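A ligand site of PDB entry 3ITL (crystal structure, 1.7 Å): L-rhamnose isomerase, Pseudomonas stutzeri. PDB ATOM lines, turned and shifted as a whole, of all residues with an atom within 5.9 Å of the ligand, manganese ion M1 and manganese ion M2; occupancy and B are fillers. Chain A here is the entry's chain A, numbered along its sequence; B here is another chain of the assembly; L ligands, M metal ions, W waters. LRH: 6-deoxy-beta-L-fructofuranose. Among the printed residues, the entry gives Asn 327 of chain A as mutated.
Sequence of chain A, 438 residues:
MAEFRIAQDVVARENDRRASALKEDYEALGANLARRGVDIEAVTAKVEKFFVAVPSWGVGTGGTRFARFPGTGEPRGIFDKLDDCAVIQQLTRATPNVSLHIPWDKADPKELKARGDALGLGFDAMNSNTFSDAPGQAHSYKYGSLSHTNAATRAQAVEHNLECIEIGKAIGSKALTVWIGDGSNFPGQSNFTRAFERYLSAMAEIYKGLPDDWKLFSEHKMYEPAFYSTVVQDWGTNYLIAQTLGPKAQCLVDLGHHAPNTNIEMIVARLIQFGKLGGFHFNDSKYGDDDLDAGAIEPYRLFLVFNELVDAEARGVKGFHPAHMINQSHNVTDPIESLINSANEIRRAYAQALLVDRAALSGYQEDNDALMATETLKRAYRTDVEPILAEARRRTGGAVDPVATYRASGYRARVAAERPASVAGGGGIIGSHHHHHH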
ATOM      1  N   TRP A  57       4.126   4.969  -1.292  1.00  0.00           N
ATOM      2  CA  TRP A  57       4.333   4.982  -2.734  1.00  0.00           C
ATOM      3  C   TRP A  57       3.438   5.949  -3.506  1.00  0.00           C
ATOM      4  O   TRP A  57       3.588   6.107  -4.719  1.00  0.00           O
ATOM      5  CB  TRP A  57       4.155   3.561  -3.297  1.00  0.00           C
ATOM      6  CG  TRP A  57       2.782   2.988  -3.095  1.00  0.00           C
ATOM      7  CD1 TRP A  57       1.739   3.027  -3.974  1.00  0.00           C
ATOM      8  CD2 TRP A  57       2.313   2.277  -1.944  1.00  0.00           C
ATOM      9  NE1 TRP A  57       0.640   2.397  -3.428  1.00  0.00           N
ATOM     10  CE2 TRP A  57       0.967   1.926  -2.193  1.00  0.00           C
ATOM     11  CE3 TRP A  57       2.894   1.911  -0.727  1.00  0.00           C
ATOM     12  CZ2 TRP A  57       0.197   1.226  -1.258  1.00  0.00           C
ATOM     13  CZ3 TRP A  57       2.131   1.212   0.202  1.00  0.00           C
ATOM     14  CH2 TRP A  57       0.790   0.878  -0.070  1.00  0.00           C
ATOM     15  N   HIS A 101       5.694  -0.326   1.679  1.00  0.00           N
ATOM     16  CA  HIS A 101       5.687  -1.372   0.669  1.00  0.00           C
ATOM     17  C   HIS A 101       7.127  -1.890   0.593  1.00  0.00           C
ATOM     18  O   HIS A 101       8.064  -1.119   0.445  1.00  0.00           O
ATOM     19  CB  HIS A 101       5.250  -0.795  -0.687  1.00  0.00           C
ATOM     20  CG  HIS A 101       4.383  -1.722  -1.482  1.00  0.00           C
ATOM     21  ND1 HIS A 101       4.800  -2.964  -1.893  1.00  0.00           N
ATOM     22  CD2 HIS A 101       3.102  -1.588  -1.904  1.00  0.00           C
ATOM     23  CE1 HIS A 101       3.815  -3.568  -2.546  1.00  0.00           C
ATOM     24  NE2 HIS A 101       2.771  -2.751  -2.569  1.00  0.00           N
ATOM     25  N   TRP A 104      10.334  -1.775  -1.863  1.00  0.00           N
ATOM     26  CA  TRP A 104      10.511  -0.363  -2.180  1.00  0.00           C
ATOM     27  C   TRP A 104      11.014   0.447  -0.995  1.00  0.00           C
ATOM     28  O   TRP A 104      11.932   1.259  -1.144  1.00  0.00           O
ATOM     29  CB  TRP A 104       9.201   0.277  -2.665  1.00  0.00           C
ATOM     30  CG  TRP A 104       8.645  -0.327  -3.908  1.00  0.00           C
ATOM     31  CD1 TRP A 104       9.322  -1.048  -4.856  1.00  0.00           C
ATOM     32  CD2 TRP A 104       7.291  -0.217  -4.370  1.00  0.00           C
ATOM     33  NE1 TRP A 104       8.473  -1.404  -5.878  1.00  0.00           N
ATOM     34  CE2 TRP A 104       7.225  -0.906  -5.604  1.00  0.00           C
ATOM     35  CE3 TRP A 104       6.134   0.387  -3.856  1.00  0.00           C
ATOM     36  CZ2 TRP A 104       6.031  -1.008  -6.340  1.00  0.00           C
ATOM     37  CZ3 TRP A 104       4.958   0.285  -4.588  1.00  0.00           C
ATOM     38  CH2 TRP A 104       4.909  -0.402  -5.818  1.00  0.00           C
ATOM     39  N   ASN A 127       2.922  -3.993   3.295  1.00  0.00           N
ATOM     40  CA  ASN A 127       2.506  -4.483   1.984  1.00  0.00           C
ATOM     41  C   ASN A 127       3.674  -5.252   1.384  1.00  0.00           C
ATOM     42  O   ASN A 127       4.774  -4.712   1.264  1.00  0.00           O
ATOM     43  CB  ASN A 127       2.150  -3.316   1.063  1.00  0.00           C
ATOM     44  CG  ASN A 127       0.902  -2.587   1.506  1.00  0.00           C
ATOM     45  OD1 ASN A 127      -0.220  -2.949   1.144  1.00  0.00           O
ATOM     46  ND2 ASN A 127       1.074  -1.552   2.322  1.00  0.00           N
ATOM     47  N   SER A 128       3.442  -6.511   1.011  1.00  0.00           N
ATOM     48  CA  SER A 128       4.485  -7.324   0.400  1.00  0.00           C
ATOM     49  C   SER A 128       4.458  -7.118  -1.110  1.00  0.00           C
ATOM     50  O   SER A 128       3.462  -6.677  -1.665  1.00  0.00           O
ATOM     51  CB  SER A 128       4.262  -8.804   0.731  1.00  0.00           C
ATOM     52  OG  SER A 128       2.965  -9.227   0.344  1.00  0.00           O
ATOM     53  N   PHE A 131       5.050  -9.203  -7.057  1.00  0.00           N
ATOM     54  CA  PHE A 131       4.468  -8.973  -8.386  1.00  0.00           C
ATOM     55  C   PHE A 131       5.512  -8.303  -9.290  1.00  0.00           C
ATOM     56  O   PHE A 131       5.205  -7.860 -10.401  1.00  0.00           O
ATOM     57  CB  PHE A 131       3.202  -8.117  -8.277  1.00  0.00           C
ATOM     58  CG  PHE A 131       3.376  -6.830  -7.512  1.00  0.00           C
ATOM     59  CD1 PHE A 131       3.989  -5.730  -8.111  1.00  0.00           C
ATOM     60  CD2 PHE A 131       2.903  -6.713  -6.212  1.00  0.00           C
ATOM     61  CE1 PHE A 131       4.131  -4.540  -7.412  1.00  0.00           C
ATOM     62  CE2 PHE A 131       3.048  -5.524  -5.496  1.00  0.00           C
ATOM     63  CZ  PHE A 131       3.664  -4.430  -6.107  1.00  0.00           C
ATOM     64  N   THR A 177      -0.719  -6.899   4.289  1.00  0.00           N
ATOM     65  CA  THR A 177      -1.651  -6.950   3.159  1.00  0.00           C
ATOM     66  C   THR A 177      -0.943  -7.685   2.032  1.00  0.00           C
ATOM     67  O   THR A 177       0.184  -7.349   1.671  1.00  0.00           O
ATOM     68  CB  THR A 177      -2.029  -5.555   2.655  1.00  0.00           C
ATOM     69  OG1 THR A 177      -2.780  -4.858   3.668  1.00  0.00           O
ATOM     70  CG2 THR A 177      -2.882  -5.661   1.379  1.00  0.00           C
ATOM     71  N   TRP A 179      -1.246  -8.625  -1.848  1.00  0.00           N
ATOM     72  CA  TRP A 179      -1.843  -8.482  -3.162  1.00  0.00           C
ATOM     73  C   TRP A 179      -0.799  -9.002  -4.136  1.00  0.00           C
ATOM     74  O   TRP A 179       0.354  -8.582  -4.094  1.00  0.00           O
ATOM     75  CB  TRP A 179      -2.137  -7.032  -3.534  1.00  0.00           C
ATOM     76  CG  TRP A 179      -2.583  -6.948  -4.974  1.00  0.00           C
ATOM     77  CD1 TRP A 179      -3.772  -7.391  -5.485  1.00  0.00           C
ATOM     78  CD2 TRP A 179      -1.793  -6.533  -6.096  1.00  0.00           C
ATOM     79  NE1 TRP A 179      -3.764  -7.283  -6.865  1.00  0.00           N
ATOM     80  CE2 TRP A 179      -2.569  -6.761  -7.259  1.00  0.00           C
ATOM     81  CE3 TRP A 179      -0.505  -5.992  -6.232  1.00  0.00           C
ATOM     82  CZ2 TRP A 179      -2.097  -6.453  -8.542  1.00  0.00           C
ATOM     83  CZ3 TRP A 179      -0.040  -5.699  -7.509  1.00  0.00           C
ATOM     84  CH2 TRP A 179      -0.822  -5.930  -8.648  1.00  0.00           C
ATOM     85  N   GLU A 219      -6.042  -9.436  -0.766  1.00  0.00           N
ATOM     86  CA  GLU A 219      -6.762  -8.466  -1.598  1.00  0.00           C
ATOM     87  C   GLU A 219      -7.115  -8.996  -2.994  1.00  0.00           C
ATOM     88  O   GLU A 219      -6.234  -9.392  -3.756  1.00  0.00           O
ATOM     89  CB  GLU A 219      -5.902  -7.198  -1.727  1.00  0.00           C
ATOM     90  CG  GLU A 219      -6.457  -6.144  -2.678  1.00  0.00           C
ATOM     91  CD  GLU A 219      -5.550  -4.925  -2.763  1.00  0.00           C
ATOM     92  OE1 GLU A 219      -4.399  -5.002  -2.282  1.00  0.00           O
ATOM     93  OE2 GLU A 219      -5.997  -3.895  -3.308  1.00  0.00           O
ATOM     94  N   LYS A 221      -8.635  -8.787  -6.952  1.00  0.00           N
ATOM     95  CA  LYS A 221      -8.576  -7.867  -8.080  1.00  0.00           C
ATOM     96  C   LYS A 221      -9.021  -8.655  -9.316  1.00  0.00           C
ATOM     97  O   LYS A 221      -8.493  -9.720  -9.591  1.00  0.00           O
ATOM     98  CB  LYS A 221      -7.172  -7.328  -8.281  1.00  0.00           C
ATOM     99  CG  LYS A 221      -7.102  -6.186  -9.287  1.00  0.00           C
ATOM    100  CD  LYS A 221      -5.719  -5.578  -9.366  1.00  0.00           C
ATOM    101  CE  LYS A 221      -5.690  -4.413 -10.355  1.00  0.00           C
ATOM    102  NZ  LYS A 221      -4.310  -3.903 -10.573  1.00  0.00           N
ATOM    103  N   GLU A 224      -5.410  -7.343 -14.192  1.00  0.00           N
ATOM    104  CA  GLU A 224      -4.240  -6.457 -14.197  1.00  0.00           C
ATOM    105  C   GLU A 224      -3.360  -6.756 -12.982  1.00  0.00           C
ATOM    106  O   GLU A 224      -3.746  -6.459 -11.845  1.00  0.00           O
ATOM    107  CB  GLU A 224      -4.612  -4.965 -14.197  1.00  0.00           C
ATOM    108  CG  GLU A 224      -3.356  -4.092 -14.335  1.00  0.00           C
ATOM    109  CD  GLU A 224      -3.561  -2.630 -14.000  1.00  0.00           C
ATOM    110  OE1 GLU A 224      -4.328  -2.328 -13.064  1.00  0.00           O
ATOM    111  OE2 GLU A 224      -2.908  -1.779 -14.652  1.00  0.00           O
ATOM    112  N   LEU A 252      -9.409  -7.585   2.104  1.00  0.00           N
ATOM    113  CA  LEU A 252      -9.225  -6.163   1.857  1.00  0.00           C
ATOM    114  C   LEU A 252      -9.967  -5.820   0.575  1.00  0.00           C
ATOM    115  O   LEU A 252      -9.786  -6.481  -0.453  1.00  0.00           O
ATOM    116  CB  LEU A 252      -7.743  -5.814   1.729  1.00  0.00           C
ATOM    117  CG  LEU A 252      -7.482  -4.306   1.687  1.00  0.00           C
ATOM    118  CD1 LEU A 252      -6.398  -3.931   2.689  1.00  0.00           C
ATOM    119  CD2 LEU A 252      -7.111  -3.892   0.276  1.00  0.00           C
ATOM    120  N   ASP A 254     -10.543  -3.153  -2.335  1.00  0.00           N
ATOM    121  CA  ASP A 254     -10.009  -1.988  -3.044  1.00  0.00           C
ATOM    122  C   ASP A 254     -11.112  -1.578  -4.025  1.00  0.00           C
ATOM    123  O   ASP A 254     -11.480  -2.340  -4.914  1.00  0.00           O
ATOM    124  CB  ASP A 254      -8.714  -2.369  -3.777  1.00  0.00           C
ATOM    125  CG  ASP A 254      -8.020  -1.176  -4.392  1.00  0.00           C
ATOM    126  OD1 ASP A 254      -6.781  -1.028  -4.217  1.00  0.00           O
ATOM    127  OD2 ASP A 254      -8.697  -0.376  -5.063  1.00  0.00           O
ATOM    128  N   HIS A 257     -11.037  -2.426  -7.890  1.00  0.00           N
ATOM    129  CA  HIS A 257     -10.735  -3.790  -8.312  1.00  0.00           C
ATOM    130  C   HIS A 257     -11.935  -4.662  -8.687  1.00  0.00           C
ATOM    131  O   HIS A 257     -11.817  -5.889  -8.691  1.00  0.00           O
ATOM    132  CB  HIS A 257      -9.941  -4.515  -7.226  1.00  0.00           C
ATOM    133  CG  HIS A 257      -8.573  -3.962  -6.998  1.00  0.00           C
ATOM    134  ND1 HIS A 257      -7.630  -4.627  -6.233  1.00  0.00           N
ATOM    135  CD2 HIS A 257      -7.977  -2.831  -7.430  1.00  0.00           C
ATOM    136  CE1 HIS A 257      -6.505  -3.923  -6.226  1.00  0.00           C
ATOM    137  NE2 HIS A 257      -6.688  -2.833  -6.949  1.00  0.00           N
ATOM    138  N   HIS A 281      -9.019  -0.078   0.588  1.00  0.00           N
ATOM    139  CA  HIS A 281      -8.029   0.644  -0.202  1.00  0.00           C
ATOM    140  C   HIS A 281      -8.936   1.621  -0.925  1.00  0.00           C
ATOM    141  O   HIS A 281      -9.735   1.236  -1.774  1.00  0.00           O
ATOM    142  CB  HIS A 281      -7.301  -0.255  -1.195  1.00  0.00           C
ATOM    143  CG  HIS A 281      -5.990  -0.782  -0.692  1.00  0.00           C
ATOM    144  ND1 HIS A 281      -5.055  -1.363  -1.511  1.00  0.00           N
ATOM    145  CD2 HIS A 281      -5.479  -0.807   0.557  1.00  0.00           C
ATOM    146  CE1 HIS A 281      -4.008  -1.733  -0.784  1.00  0.00           C
ATOM    147  NE2 HIS A 281      -4.239  -1.410   0.470  1.00  0.00           N
ATOM    148  N   ASN A 283      -9.853   4.925  -3.308  1.00  0.00           N
ATOM    149  CA  ASN A 283      -9.463   5.593  -4.539  1.00  0.00           C
ATOM    150  C   ASN A 283     -10.748   5.702  -5.346  1.00  0.00           C
ATOM    151  O   ASN A 283     -11.807   5.265  -4.894  1.00  0.00           O
ATOM    152  CB  ASN A 283      -8.418   4.762  -5.303  1.00  0.00           C
ATOM    153  CG  ASN A 283      -8.813   3.299  -5.464  1.00  0.00           C
ATOM    154  OD1 ASN A 283      -9.855   2.972  -6.049  1.00  0.00           O
ATOM    155  ND2 ASN A 283      -7.972   2.407  -4.939  1.00  0.00           N
ATOM    156  N   ASP A 289      -8.855  -0.149 -12.778  1.00  0.00           N
ATOM    157  CA  ASP A 289      -8.231   0.175 -11.500  1.00  0.00           C
ATOM    158  C   ASP A 289      -7.473   1.478 -11.755  1.00  0.00           C
ATOM    159  O   ASP A 289      -6.235   1.509 -11.750  1.00  0.00           O
ATOM    160  CB  ASP A 289      -7.279  -0.951 -11.081  1.00  0.00           C
ATOM    161  CG  ASP A 289      -6.710  -0.746  -9.686  1.00  0.00           C
ATOM    162  OD1 ASP A 289      -7.365  -0.072  -8.871  1.00  0.00           O
ATOM    163  OD2 ASP A 289      -5.604  -1.276  -9.399  1.00  0.00           O
ATOM    164  N   ASP A 291      -7.106   4.202  -9.987  1.00  0.00           N
ATOM    165  CA  ASP A 291      -6.364   4.772  -8.872  1.00  0.00           C
ATOM    166  C   ASP A 291      -6.393   6.292  -8.769  1.00  0.00           C
ATOM    167  O   ASP A 291      -5.413   6.925  -8.376  1.00  0.00           O
ATOM    168  CB  ASP A 291      -4.912   4.290  -8.930  1.00  0.00           C
ATOM    169  CG  ASP A 291      -4.766   2.829  -8.559  1.00  0.00           C
ATOM    170  OD1 ASP A 291      -5.594   2.374  -7.744  1.00  0.00           O
ATOM    171  OD2 ASP A 291      -3.852   2.141  -9.056  1.00  0.00           O
ATOM    172  N   ASN A 327      -5.067   4.126  -1.466  1.00  0.00           N
ATOM    173  CA  ASN A 327      -4.186   3.449  -2.406  1.00  0.00           C
ATOM    174  C   ASN A 327      -4.483   4.100  -3.746  1.00  0.00           C
ATOM    175  O   ASN A 327      -5.421   3.722  -4.433  1.00  0.00           O
ATOM    176  CB  ASN A 327      -4.476   1.946  -2.471  1.00  0.00           C
ATOM    177  CG  ASN A 327      -3.460   1.209  -3.314  1.00  0.00           C
ATOM    178  OD1 ASN A 327      -2.261   1.263  -3.046  1.00  0.00           O
ATOM    179  ND2 ASN A 327      -3.928   0.513  -4.351  1.00  0.00           N
ATOM    180  N   ARG B  65       2.106  -1.722 -15.781  1.00  0.00           N
ATOM    181  CA  ARG B  65       2.650  -0.660 -14.937  1.00  0.00           C
ATOM    182  C   ARG B  65       3.271  -1.225 -13.659  1.00  0.00           C
ATOM    183  O   ARG B  65       4.002  -0.523 -12.960  1.00  0.00           O
ATOM    184  CB  ARG B  65       1.566   0.357 -14.584  1.00  0.00           C
ATOM    185  CG  ARG B  65       0.354  -0.219 -13.900  1.00  0.00           C
ATOM    186  CD  ARG B  65      -0.567   0.879 -13.381  1.00  0.00           C
ATOM    187  NE  ARG B  65      -1.812   0.305 -12.885  1.00  0.00           N
ATOM    188  CZ  ARG B  65      -2.535   0.799 -11.885  1.00  0.00           C
ATOM    189  NH1 ARG B  65      -2.152   1.897 -11.248  1.00  0.00           N
ATOM    190  NH2 ARG B  65      -3.646   0.179 -11.518  1.00  0.00           N
ATOM    191  N   PHE B  66       2.988  -2.487 -13.363  1.00  0.00           N
ATOM    192  CA  PHE B  66       3.515  -3.125 -12.171  1.00  0.00           C
ATOM    193  C   PHE B  66       4.871  -3.797 -12.380  1.00  0.00           C
ATOM    194  O   PHE B  66       5.684  -3.835 -11.456  1.00  0.00           O
ATOM    195  CB  PHE B  66       2.511  -4.153 -11.622  1.00  0.00           C
ATOM    196  CG  PHE B  66       1.256  -3.529 -11.096  1.00  0.00           C
ATOM    197  CD1 PHE B  66       1.265  -2.859  -9.868  1.00  0.00           C
ATOM    198  CD2 PHE B  66       0.092  -3.528 -11.859  1.00  0.00           C
ATOM    199  CE1 PHE B  66       0.131  -2.207  -9.413  1.00  0.00           C
ATOM    200  CE2 PHE B  66      -1.051  -2.876 -11.414  1.00  0.00           C
ATOM    201  CZ  PHE B  66      -1.037  -2.213 -10.181  1.00  0.00           C
HETATM  202  C1  LRH L   1      -2.908  -3.599  -6.777  1.00  0.00           C
HETATM  203  C2  LRH L   1      -2.752  -2.605  -5.653  1.00  0.00           C
HETATM  204  C3  LRH L   1      -2.216  -3.193  -4.338  1.00  0.00           C
HETATM  205  C4  LRH L   1      -0.922  -2.430  -4.055  1.00  0.00           C
HETATM  206  C5  LRH L   1      -0.577  -1.745  -5.379  1.00  0.00           C
HETATM  207  C6  LRH L   1      -0.002  -0.355  -5.207  1.00  0.00           C
HETATM  208  O1  LRH L   1      -3.462  -2.966  -7.925  1.00  0.00           O
HETATM  209  O2  LRH L   1      -4.000  -1.962  -5.418  1.00  0.00           O
HETATM  210  O3  LRH L   1      -3.138  -2.953  -3.282  1.00  0.00           O
HETATM  211  O4  LRH L   1       0.112  -3.332  -3.692  1.00  0.00           O
HETATM  212  O5  LRH L   1      -1.807  -1.617  -6.092  1.00  0.00           O
HETATM  213 MN    MN M   1      -5.084  -2.060  -3.582  1.00  0.00          MN
HETATM  214 MN    MN M   2      -5.073  -1.449  -7.333  1.00  0.00          MN
HETATM  215  O   HOH W   1      -5.733   0.339  -6.388  1.00  0.00           O
HETATM  216  O   HOH W   2      -3.401  -0.220  -7.901  1.00  0.00           O
HETATM  217  O   HOH W   3      -0.553  -4.456  -1.296  1.00  0.00           O
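Manganese ion M2 is bound by water W1 (2.1 Å), the side-chain carboxylate (OD2) of Asp 289 (2.1 Å), water W2 (2.2 Å), a ring nitrogen (NE2) of His 257 (2.2 Å), an oxygen (O2) of the ligand (2.3 Å) and an oxygen (O1) of the ligand (2.3 Å).
Manganese ion M2 has six donor atoms within binding distance.
Manganese ion M1 is bound by OE2 of Glu 219 (2.1 Å).
The side-chain carboxylate (OD1) of Asp 254 is bound to manganese ion M1, 2.1 Å away.
O2 of the ligand binds manganese ion M1 (2.1 Å).
Manganese ion M1 is bound by an oxygen (O3) of the ligand (2.2 Å).
ND1 of His 281 is bound to manganese ion M1 (2.2 Å).
Manganese ion M1 has five donor atoms within binding distance.
Slightly farther from manganese ion M1 lies ND2 of Asn 327 (2.9 Å).
A ring nitrogen (ND1) of His 257 lies close to the side-chain carboxylate (OE2) of Glu 219 (3.4 Å).
ND2 of Asn 327 lies close to OD1 of Asp 254 (3.2 Å).
The side-chain carboxylate (OD2) of Asp 289 lies close to the side-chain amino group (NZ) of Lys 221 (3.2 Å).
OD2 of Asp 254 is in hydrogen-bond range of ND2 of Asn 283 (2.9 Å).
The indole nitrogen of Trp 57 sits close to the side-chain amide oxygen of Asn 327 (3.1 Å).
NH1 of Arg 65 of chain B is in salt-bridge range of OD2 of Asp 291, 2.8 Å away.
The backbone carbonyl oxygen of Asn 327 sits at hydrogen-bond distance from the side-chain amide nitrogen of Asn 283, at 2.9 Å.
NZ of Lys 221 is in salt-bridge range of OE1 of Glu 224.
Water W2 lies within hydrogen-bond range of OD2 of Asp 291 (2.7 Å) and O5 of the ligand (2.8 Å).
Water W3 lies within hydrogen-bond range of O4 of the ligand and OD1 of Asn 127.
Asp 291 touches manganese ion M2 (OD1 to MN, 3.9 Å).
The nearest printed residue that does not touch manganese ion M2 is Lys 221 (4.1 Å).
Within 4 Å of manganese ion M1: Glu 219, Asp 254, His 257, His 281 and Asn 327.
The nearest printed residue that does not touch manganese ion M1 is Leu 252 (4.7 Å).
O5 of the ligand is in hydrogen-bond range of ND2 of Asn 327 (3.5 Å).
NZ of Lys 221 sits close to O1 of the ligand (2.9 Å).
An oxygen (O4) of the ligand sits at hydrogen-bond distance from a ring nitrogen (NE2) of His 101 (2.9 Å).
Trp 57 touches the ligand.
Trp 179 touches the ligand (CD2 to C1, 3.2 Å).
Phe 66 of chain B touches the ligand (CZ to O1, 3.4 Å).
Within 4 Å of the ligand: Trp 57, His 101, Trp 179, Glu 219, Lys 221, Asp 254, His 257, His 281, Asp 289, Asn 327 and Phe 66 of chain B.
Along chain A the residues within 4 Å of the ligand span positions 57 to 327.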
